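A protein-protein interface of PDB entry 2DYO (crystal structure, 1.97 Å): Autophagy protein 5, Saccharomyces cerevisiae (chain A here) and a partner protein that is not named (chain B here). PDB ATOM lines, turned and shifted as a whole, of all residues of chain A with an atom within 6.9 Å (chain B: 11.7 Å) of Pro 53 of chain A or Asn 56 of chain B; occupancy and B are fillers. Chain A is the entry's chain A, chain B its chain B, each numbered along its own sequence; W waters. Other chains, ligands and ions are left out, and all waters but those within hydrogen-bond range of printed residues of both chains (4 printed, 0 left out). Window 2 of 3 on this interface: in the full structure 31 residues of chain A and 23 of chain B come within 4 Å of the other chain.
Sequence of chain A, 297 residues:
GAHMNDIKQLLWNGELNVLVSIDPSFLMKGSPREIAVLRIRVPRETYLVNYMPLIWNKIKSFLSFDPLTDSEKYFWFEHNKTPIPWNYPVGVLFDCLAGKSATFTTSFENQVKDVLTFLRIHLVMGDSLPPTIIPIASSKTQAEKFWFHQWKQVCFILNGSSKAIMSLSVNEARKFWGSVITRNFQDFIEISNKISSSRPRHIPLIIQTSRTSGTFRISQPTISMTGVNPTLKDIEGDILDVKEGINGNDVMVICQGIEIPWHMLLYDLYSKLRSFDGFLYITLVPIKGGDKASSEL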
ATOM      1  N   LEU A  48       1.478 -18.125 -13.346  1.00  0.00           N
ATOM      2  CA  LEU A  48       0.335 -17.599 -12.603  1.00  0.00           C
ATOM      3  C   LEU A  48      -0.796 -17.212 -13.548  1.00  0.00           C
ATOM      4  O   LEU A  48      -1.968 -17.300 -13.209  1.00  0.00           O
ATOM      5  CB  LEU A  48       0.756 -16.368 -11.782  1.00  0.00           C
ATOM      6  CG  LEU A  48       1.672 -16.606 -10.573  1.00  0.00           C
ATOM      7  CD1 LEU A  48       2.133 -15.258 -10.019  1.00  0.00           C
ATOM      8  CD2 LEU A  48       0.934 -17.395  -9.510  1.00  0.00           C
ATOM      9  N   VAL A  49      -0.421 -16.768 -14.739  1.00  0.00           N
ATOM     10  CA  VAL A  49      -1.379 -16.346 -15.746  1.00  0.00           C
ATOM     11  C   VAL A  49      -2.323 -17.464 -16.205  1.00  0.00           C
ATOM     12  O   VAL A  49      -3.394 -17.200 -16.762  1.00  0.00           O
ATOM     13  CB  VAL A  49      -0.631 -15.714 -16.926  1.00  0.00           C
ATOM     14  CG1 VAL A  49      -0.403 -16.718 -18.030  1.00  0.00           C
ATOM     15  CG2 VAL A  49      -1.358 -14.464 -17.386  1.00  0.00           C
ATOM     16  N   ASN A  50      -1.949 -18.714 -15.952  1.00  0.00           N
ATOM     17  CA  ASN A  50      -2.812 -19.834 -16.315  1.00  0.00           C
ATOM     18  C   ASN A  50      -4.053 -19.888 -15.418  1.00  0.00           C
ATOM     19  O   ASN A  50      -4.947 -20.723 -15.620  1.00  0.00           O
ATOM     20  CB  ASN A  50      -2.039 -21.148 -16.215  1.00  0.00           C
ATOM     21  CG  ASN A  50      -1.046 -21.305 -17.345  1.00  0.00           C
ATOM     22  OD1 ASN A  50      -0.153 -22.151 -17.308  1.00  0.00           O
ATOM     23  ND2 ASN A  50      -1.218 -20.490 -18.377  1.00  0.00           N
ATOM     24  N   TYR A  51      -4.113 -18.996 -14.433  1.00  0.00           N
ATOM     25  CA  TYR A  51      -5.250 -18.967 -13.527  1.00  0.00           C
ATOM     26  C   TYR A  51      -6.189 -17.778 -13.728  1.00  0.00           C
ATOM     27  O   TYR A  51      -7.080 -17.543 -12.912  1.00  0.00           O
ATOM     28  CB  TYR A  51      -4.758 -19.036 -12.074  1.00  0.00           C
ATOM     29  CG  TYR A  51      -4.000 -20.316 -11.818  1.00  0.00           C
ATOM     30  CD1 TYR A  51      -2.670 -20.448 -12.213  1.00  0.00           C
ATOM     31  CD2 TYR A  51      -4.652 -21.444 -11.327  1.00  0.00           C
ATOM     32  CE1 TYR A  51      -2.015 -21.677 -12.144  1.00  0.00           C
ATOM     33  CE2 TYR A  51      -4.010 -22.675 -11.252  1.00  0.00           C
ATOM     34  CZ  TYR A  51      -2.692 -22.784 -11.669  1.00  0.00           C
ATOM     35  OH  TYR A  51      -2.079 -24.012 -11.657  1.00  0.00           O
ATOM     36  N   MET A  52      -6.003 -17.035 -14.814  1.00  0.00           N
ATOM     37  CA  MET A  52      -6.877 -15.898 -15.092  1.00  0.00           C
ATOM     38  C   MET A  52      -8.319 -16.341 -15.348  1.00  0.00           C
ATOM     39  O   MET A  52      -9.264 -15.690 -14.894  1.00  0.00           O
ATOM     40  CB  MET A  52      -6.358 -15.094 -16.288  1.00  0.00           C
ATOM     41  CG  MET A  52      -5.086 -14.327 -15.986  1.00  0.00           C
ATOM     42  SD  MET A  52      -5.163 -13.479 -14.389  1.00  0.00           S
ATOM     43  CE  MET A  52      -6.493 -12.312 -14.662  1.00  0.00           C
ATOM     44  N   PRO A  53      -8.509 -17.448 -16.089  1.00  0.00           N
ATOM     45  CA  PRO A  53      -9.874 -17.918 -16.356  1.00  0.00           C
ATOM     46  C   PRO A  53     -10.612 -18.196 -15.048  1.00  0.00           C
ATOM     47  O   PRO A  53     -11.778 -17.829 -14.883  1.00  0.00           O
ATOM     48  CB  PRO A  53      -9.644 -19.191 -17.169  1.00  0.00           C
ATOM     49  CG  PRO A  53      -8.399 -18.865 -17.937  1.00  0.00           C
ATOM     50  CD  PRO A  53      -7.529 -18.229 -16.867  1.00  0.00           C
ATOM     51  N   LEU A  54      -9.914 -18.847 -14.121  1.00  0.00           N
ATOM     52  CA  LEU A  54     -10.472 -19.184 -12.817  1.00  0.00           C
ATOM     53  C   LEU A  54     -10.831 -17.909 -12.054  1.00  0.00           C
ATOM     54  O   LEU A  54     -11.870 -17.833 -11.396  1.00  0.00           O
ATOM     55  CB  LEU A  54      -9.453 -20.000 -12.015  1.00  0.00           C
ATOM     56  CG  LEU A  54      -9.856 -20.457 -10.613  1.00  0.00           C
ATOM     57  CD1 LEU A  54     -10.914 -21.542 -10.721  1.00  0.00           C
ATOM     58  CD2 LEU A  54      -8.632 -20.987  -9.872  1.00  0.00           C
ATOM     59  N   ILE A  55      -9.960 -16.911 -12.143  1.00  0.00           N
ATOM     60  CA  ILE A  55     -10.183 -15.640 -11.469  1.00  0.00           C
ATOM     61  C   ILE A  55     -11.376 -14.894 -12.066  1.00  0.00           C
ATOM     62  O   ILE A  55     -12.310 -14.510 -11.352  1.00  0.00           O
ATOM     63  CB  ILE A  55      -8.933 -14.739 -11.564  1.00  0.00           C
ATOM     64  CG1 ILE A  55      -7.780 -15.372 -10.778  1.00  0.00           C
ATOM     65  CG2 ILE A  55      -9.246 -13.343 -11.032  1.00  0.00           C
ATOM     66  CD1 ILE A  55      -6.496 -14.566 -10.808  1.00  0.00           C
ATOM     67  N   TRP A  56     -11.345 -14.686 -13.376  1.00  0.00           N
ATOM     68  CA  TRP A  56     -12.424 -13.983 -14.048  1.00  0.00           C
ATOM     69  C   TRP A  56     -13.781 -14.632 -13.787  1.00  0.00           C
ATOM     70  O   TRP A  56     -14.745 -13.946 -13.444  1.00  0.00           O
ATOM     71  CB  TRP A  56     -12.148 -13.921 -15.553  1.00  0.00           C
ATOM     72  CG  TRP A  56     -11.030 -12.979 -15.919  1.00  0.00           C
ATOM     73  CD1 TRP A  56      -9.968 -13.243 -16.737  1.00  0.00           C
ATOM     74  CD2 TRP A  56     -10.879 -11.620 -15.493  1.00  0.00           C
ATOM     75  NE1 TRP A  56      -9.165 -12.133 -16.847  1.00  0.00           N
ATOM     76  CE2 TRP A  56      -9.702 -11.121 -16.095  1.00  0.00           C
ATOM     77  CE3 TRP A  56     -11.627 -10.773 -14.665  1.00  0.00           C
ATOM     78  CZ2 TRP A  56      -9.252  -9.813 -15.891  1.00  0.00           C
ATOM     79  CZ3 TRP A  56     -11.179  -9.469 -14.463  1.00  0.00           C
ATOM     80  CH2 TRP A  56     -10.002  -9.005 -15.076  1.00  0.00           C
ATOM     81  N   ASN A  57     -13.855 -15.951 -13.933  1.00  0.00           N
ATOM     82  CA  ASN A  57     -15.110 -16.662 -13.714  1.00  0.00           C
ATOM     83  C   ASN A  57     -15.706 -16.432 -12.328  1.00  0.00           C
ATOM     84  O   ASN A  57     -16.917 -16.519 -12.152  1.00  0.00           O
ATOM     85  CB  ASN A  57     -14.928 -18.165 -13.921  1.00  0.00           C
ATOM     86  CG  ASN A  57     -16.199 -18.948 -13.622  1.00  0.00           C
ATOM     87  OD1 ASN A  57     -17.209 -18.801 -14.314  1.00  0.00           O
ATOM     88  ND2 ASN A  57     -16.157 -19.774 -12.584  1.00  0.00           N
ATOM     89  N   LYS A  58     -14.863 -16.137 -11.344  1.00  0.00           N
ATOM     90  CA  LYS A  58     -15.355 -15.928  -9.990  1.00  0.00           C
ATOM     91  C   LYS A  58     -15.796 -14.502  -9.688  1.00  0.00           C
ATOM     92  O   LYS A  58     -16.703 -14.294  -8.883  1.00  0.00           O
ATOM     93  CB  LYS A  58     -14.298 -16.353  -8.963  1.00  0.00           C
ATOM     94  CG  LYS A  58     -14.774 -16.199  -7.523  1.00  0.00           C
ATOM     95  CD  LYS A  58     -13.755 -16.698  -6.513  1.00  0.00           C
ATOM     96  CE  LYS A  58     -14.350 -16.678  -5.113  1.00  0.00           C
ATOM     97  NZ  LYS A  58     -13.440 -17.249  -4.086  1.00  0.00           N
ATOM     98  N   TRP A 177       2.380 -27.751 -24.909  1.00  0.00           N
ATOM     99  CA  TRP A 177       1.833 -26.730 -24.015  1.00  0.00           C
ATOM    100  C   TRP A 177       0.666 -27.303 -23.224  1.00  0.00           C
ATOM    101  O   TRP A 177       0.511 -27.033 -22.033  1.00  0.00           O
ATOM    102  CB  TRP A 177       1.337 -25.517 -24.805  1.00  0.00           C
ATOM    103  CG  TRP A 177       0.562 -24.540 -23.950  1.00  0.00           C
ATOM    104  CD1 TRP A 177      -0.770 -24.244 -24.035  1.00  0.00           C
ATOM    105  CD2 TRP A 177       1.075 -23.763 -22.863  1.00  0.00           C
ATOM    106  NE1 TRP A 177      -1.117 -23.329 -23.068  1.00  0.00           N
ATOM    107  CE2 TRP A 177      -0.002 -23.016 -22.335  1.00  0.00           C
ATOM    108  CE3 TRP A 177       2.344 -23.624 -22.285  1.00  0.00           C
ATOM    109  CZ2 TRP A 177       0.154 -22.143 -21.253  1.00  0.00           C
ATOM    110  CZ3 TRP A 177       2.496 -22.753 -21.208  1.00  0.00           C
ATOM    111  CH2 TRP A 177       1.409 -22.025 -20.707  1.00  0.00           C
ATOM    112  N   ILE A 181      -1.025 -27.564 -18.750  1.00  0.00           N
ATOM    113  CA  ILE A 181      -2.326 -27.259 -18.165  1.00  0.00           C
ATOM    114  C   ILE A 181      -2.949 -28.505 -17.546  1.00  0.00           C
ATOM    115  O   ILE A 181      -3.451 -28.465 -16.422  1.00  0.00           O
ATOM    116  CB  ILE A 181      -3.309 -26.707 -19.226  1.00  0.00           C
ATOM    117  CG1 ILE A 181      -2.687 -25.519 -19.964  1.00  0.00           C
ATOM    118  CG2 ILE A 181      -4.608 -26.294 -18.551  1.00  0.00           C
ATOM    119  CD1 ILE A 181      -2.412 -24.312 -19.090  1.00  0.00           C
ATOM    120  N   ASP B  48      -9.714 -24.429  -3.290  1.00  0.00           N
ATOM    121  CA  ASP B  48     -10.653 -23.770  -4.189  1.00  0.00           C
ATOM    122  C   ASP B  48     -10.580 -24.239  -5.639  1.00  0.00           C
ATOM    123  O   ASP B  48     -11.547 -24.078  -6.380  1.00  0.00           O
ATOM    124  CB  ASP B  48     -10.477 -22.253  -4.127  1.00  0.00           C
ATOM    125  CG  ASP B  48     -10.849 -21.683  -2.774  1.00  0.00           C
ATOM    126  OD1 ASP B  48     -11.282 -22.469  -1.900  1.00  0.00           O
ATOM    127  OD2 ASP B  48     -10.709 -20.455  -2.586  1.00  0.00           O
ATOM    128  N   ASN B  49      -9.448 -24.813  -6.050  1.00  0.00           N
ATOM    129  CA  ASN B  49      -9.296 -25.308  -7.423  1.00  0.00           C
ATOM    130  C   ASN B  49      -8.968 -26.799  -7.415  1.00  0.00           C
ATOM    131  O   ASN B  49      -8.274 -27.298  -8.302  1.00  0.00           O
ATOM    132  CB  ASN B  49      -8.178 -24.545  -8.147  1.00  0.00           C
ATOM    133  CG  ASN B  49      -6.791 -24.907  -7.630  1.00  0.00           C
ATOM    134  OD1 ASN B  49      -6.601 -25.116  -6.433  1.00  0.00           O
ATOM    135  ND2 ASN B  49      -5.812 -24.970  -8.534  1.00  0.00           N
ATOM    136  N   SER B  50      -9.474 -27.505  -6.410  1.00  0.00           N
ATOM    137  CA  SER B  50      -9.231 -28.937  -6.262  1.00  0.00           C
ATOM    138  C   SER B  50      -9.466 -29.766  -7.526  1.00  0.00           C
ATOM    139  O   SER B  50      -8.829 -30.802  -7.716  1.00  0.00           O
ATOM    140  CB  SER B  50     -10.084 -29.497  -5.117  1.00  0.00           C
ATOM    141  OG  SER B  50     -11.447 -29.143  -5.272  1.00  0.00           O
ATOM    142  N   GLY B  51     -10.370 -29.317  -8.389  1.00  0.00           N
ATOM    143  CA  GLY B  51     -10.639 -30.065  -9.607  1.00  0.00           C
ATOM    144  C   GLY B  51      -9.877 -29.581 -10.832  1.00  0.00           C
ATOM    145  O   GLY B  51      -9.974 -30.181 -11.906  1.00  0.00           O
ATOM    146  N   ALA B  52      -9.116 -28.501 -10.675  1.00  0.00           N
ATOM    147  CA  ALA B  52      -8.350 -27.932 -11.780  1.00  0.00           C
ATOM    148  C   ALA B  52      -7.013 -27.377 -11.289  1.00  0.00           C
ATOM    149  O   ALA B  52      -6.770 -26.169 -11.339  1.00  0.00           O
ATOM    150  CB  ALA B  52      -9.164 -26.825 -12.453  1.00  0.00           C
ATOM    151  N   ILE B  53      -6.148 -28.268 -10.819  1.00  0.00           N
ATOM    152  CA  ILE B  53      -4.841 -27.876 -10.305  1.00  0.00           C
ATOM    153  C   ILE B  53      -4.062 -27.011 -11.291  1.00  0.00           C
ATOM    154  O   ILE B  53      -3.566 -25.940 -10.928  1.00  0.00           O
ATOM    155  CB  ILE B  53      -3.986 -29.123  -9.955  1.00  0.00           C
ATOM    156  CG1 ILE B  53      -4.620 -29.878  -8.783  1.00  0.00           C
ATOM    157  CG2 ILE B  53      -2.557 -28.707  -9.594  1.00  0.00           C
ATOM    158  CD1 ILE B  53      -4.669 -29.088  -7.483  1.00  0.00           C
ATOM    159  N   GLY B  54      -3.973 -27.472 -12.537  1.00  0.00           N
ATOM    160  CA  GLY B  54      -3.228 -26.750 -13.555  1.00  0.00           C
ATOM    161  C   GLY B  54      -3.882 -25.525 -14.162  1.00  0.00           C
ATOM    162  O   GLY B  54      -3.326 -24.913 -15.077  1.00  0.00           O
ATOM    163  N   GLY B  55      -5.054 -25.151 -13.663  1.00  0.00           N
ATOM    164  CA  GLY B  55      -5.728 -23.988 -14.206  1.00  0.00           C
ATOM    165  C   GLY B  55      -6.546 -24.354 -15.429  1.00  0.00           C
ATOM    166  O   GLY B  55      -7.053 -25.470 -15.519  1.00  0.00           O
ATOM    167  N   ASN B  56      -6.668 -23.427 -16.375  1.00  0.00           N
ATOM    168  CA  ASN B  56      -7.455 -23.685 -17.574  1.00  0.00           C
ATOM    169  C   ASN B  56      -6.918 -22.993 -18.824  1.00  0.00           C
ATOM    170  O   ASN B  56      -6.158 -22.026 -18.741  1.00  0.00           O
ATOM    171  CB  ASN B  56      -8.908 -23.257 -17.343  1.00  0.00           C
ATOM    172  CG  ASN B  56      -9.469 -23.781 -16.033  1.00  0.00           C
ATOM    173  OD1 ASN B  56      -9.083 -23.329 -14.952  1.00  0.00           O
ATOM    174  ND2 ASN B  56     -10.375 -24.747 -16.123  1.00  0.00           N
ATOM    175  N   ILE B  57      -7.334 -23.503 -19.980  1.00  0.00           N
ATOM    176  CA  ILE B  57      -6.930 -22.966 -21.276  1.00  0.00           C
ATOM    177  C   ILE B  57      -7.355 -21.509 -21.432  1.00  0.00           C
ATOM    178  O   ILE B  57      -8.568 -21.261 -21.605  1.00  0.00           O
ATOM    179  CB  ILE B  57      -7.530 -23.808 -22.400  1.00  0.00           C
ATOM    180  OXT ILE B  57      -6.468 -20.633 -21.371  1.00  0.00           O
HETATM  181  O   HOH W   1     -12.006 -19.213  -4.845  1.00  0.00           O
HETATM  182  O   HOH W   2      -3.844 -22.148 -22.337  1.00  0.00           O
HETATM  183  O   HOH W   3      -7.809 -20.997 -14.814  1.00  0.00           O
HETATM  184  O   HOH W   4      -5.011 -29.528 -14.234  1.00  0.00           O
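The backbone NH of Asn 56 of chain B sits at hydrogen-bond distance from the backbone carbonyl oxygen of Asn 50 of chain A, 3.3 Å away.
OH of Tyr 51 of chain A sits at hydrogen-bond distance from O of Ile 53 of chain B, 2.5 Å away.
The backbone carbonyl oxygen (O) of Ala 52 of chain B lies within hydrogen-bond range of the side-chain amide nitrogen (ND2) of Asn 49 of chain B, at 3.2 Å.
The backbone carbonyl oxygen of Ile 53 of chain B lies within hydrogen-bond range of the side-chain amide nitrogen of Asn 49 of chain B (3.4 Å).
Asn 50 of chain A touches Gly 55 of chain B.
Tyr 51 of chain A touches Asn 49 of chain B.
Gly 54 of chain B touches Tyr 51 of chain A.
Tyr 51 of chain A touches Gly 55 of chain B (CE2 to N, 3.6 Å).
Asn 56 of chain B touches Pro 53 of chain A.
Leu 54 of chain A touches Asn 49 of chain B (CD2 to CB, 3.98 Å).
Ile 181 of chain A touches Gly 54 of chain B (O to CA, 3.3 Å).
Ile 181 of chain A touches Gly 55 of chain B.
CG2 of Ile 181 of chain A touches CA of Asn 56 of chain B, 3.98 Å away.
Pro 53 of chain A touches one residue of chain B.
No residue of chain B comes within 4 Å of Val 49 of chain A.
No residue of chain B comes within 4 Å of Ile 55 of chain A.
No residue of chain B comes within 4 Å of Asn 57 of chain A.
Of the printed residues of chain A, Gly 54 of chain B touches Tyr 51 and Ile 181.
Of the printed residues of chain A, Gly 55 of chain B touches Asn 50 (3.6 Å), Tyr 51 (3.6 Å) and Ile 181 (3.98 Å).
Printed residues of chain B within 4 Å of Tyr 51 of chain A: Asn 49 (3.99 Å), Ile 53 (2.5 Å), Gly 54 (3.4 Å) and Gly 55 (3.6 Å).
Printed residues of chain A within 4 Å of Asn 49 of chain B: Tyr 51 and Leu 54.
Of the printed residues of chain A, Ile 53 of chain B touches Tyr 51.
The nearest residue of chain B that does not touch Pro 53 of chain A is Ile 57 of chain B (4.3 Å).
The nearest printed residue of chain A that does not touch Asn 56 of chain B is Leu 54 of chain A (4.5 Å).
The nearest printed residue of chain B that does not touch Leu 54 of chain A is Asn 56 of chain B (4.5 Å).
Of the 13 printed residues of chain A, 5 touch a printed residue of chain B.
Hydrophobic or aromatic side chains of chain A within 4 Å of the printed part of chain B: Tyr 51, Pro 53, Leu 54 and Ile 181.
Water W1 bridges the side-chain amino group (NZ) of Lys 58 of chain A (2.5 Å) and the side-chain carboxylate (OD2) of Asp 48 of chain B (2.9 Å).
Water W3 lies within hydrogen-bond range of OD1 of Asn 56 of chain B (2.7 Å), O of Asn 50 of chain A (3.0 Å) and N of Leu 54 of chain A (3.1 Å).
Water W4 bridges N of Gly 54 of chain B and O of Ile 181 of chain A.
Water W2 bridges NE1 of Trp 177 of chain A (3.1 Å) and OXT of Ile 57 of chain B (3.2 Å).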
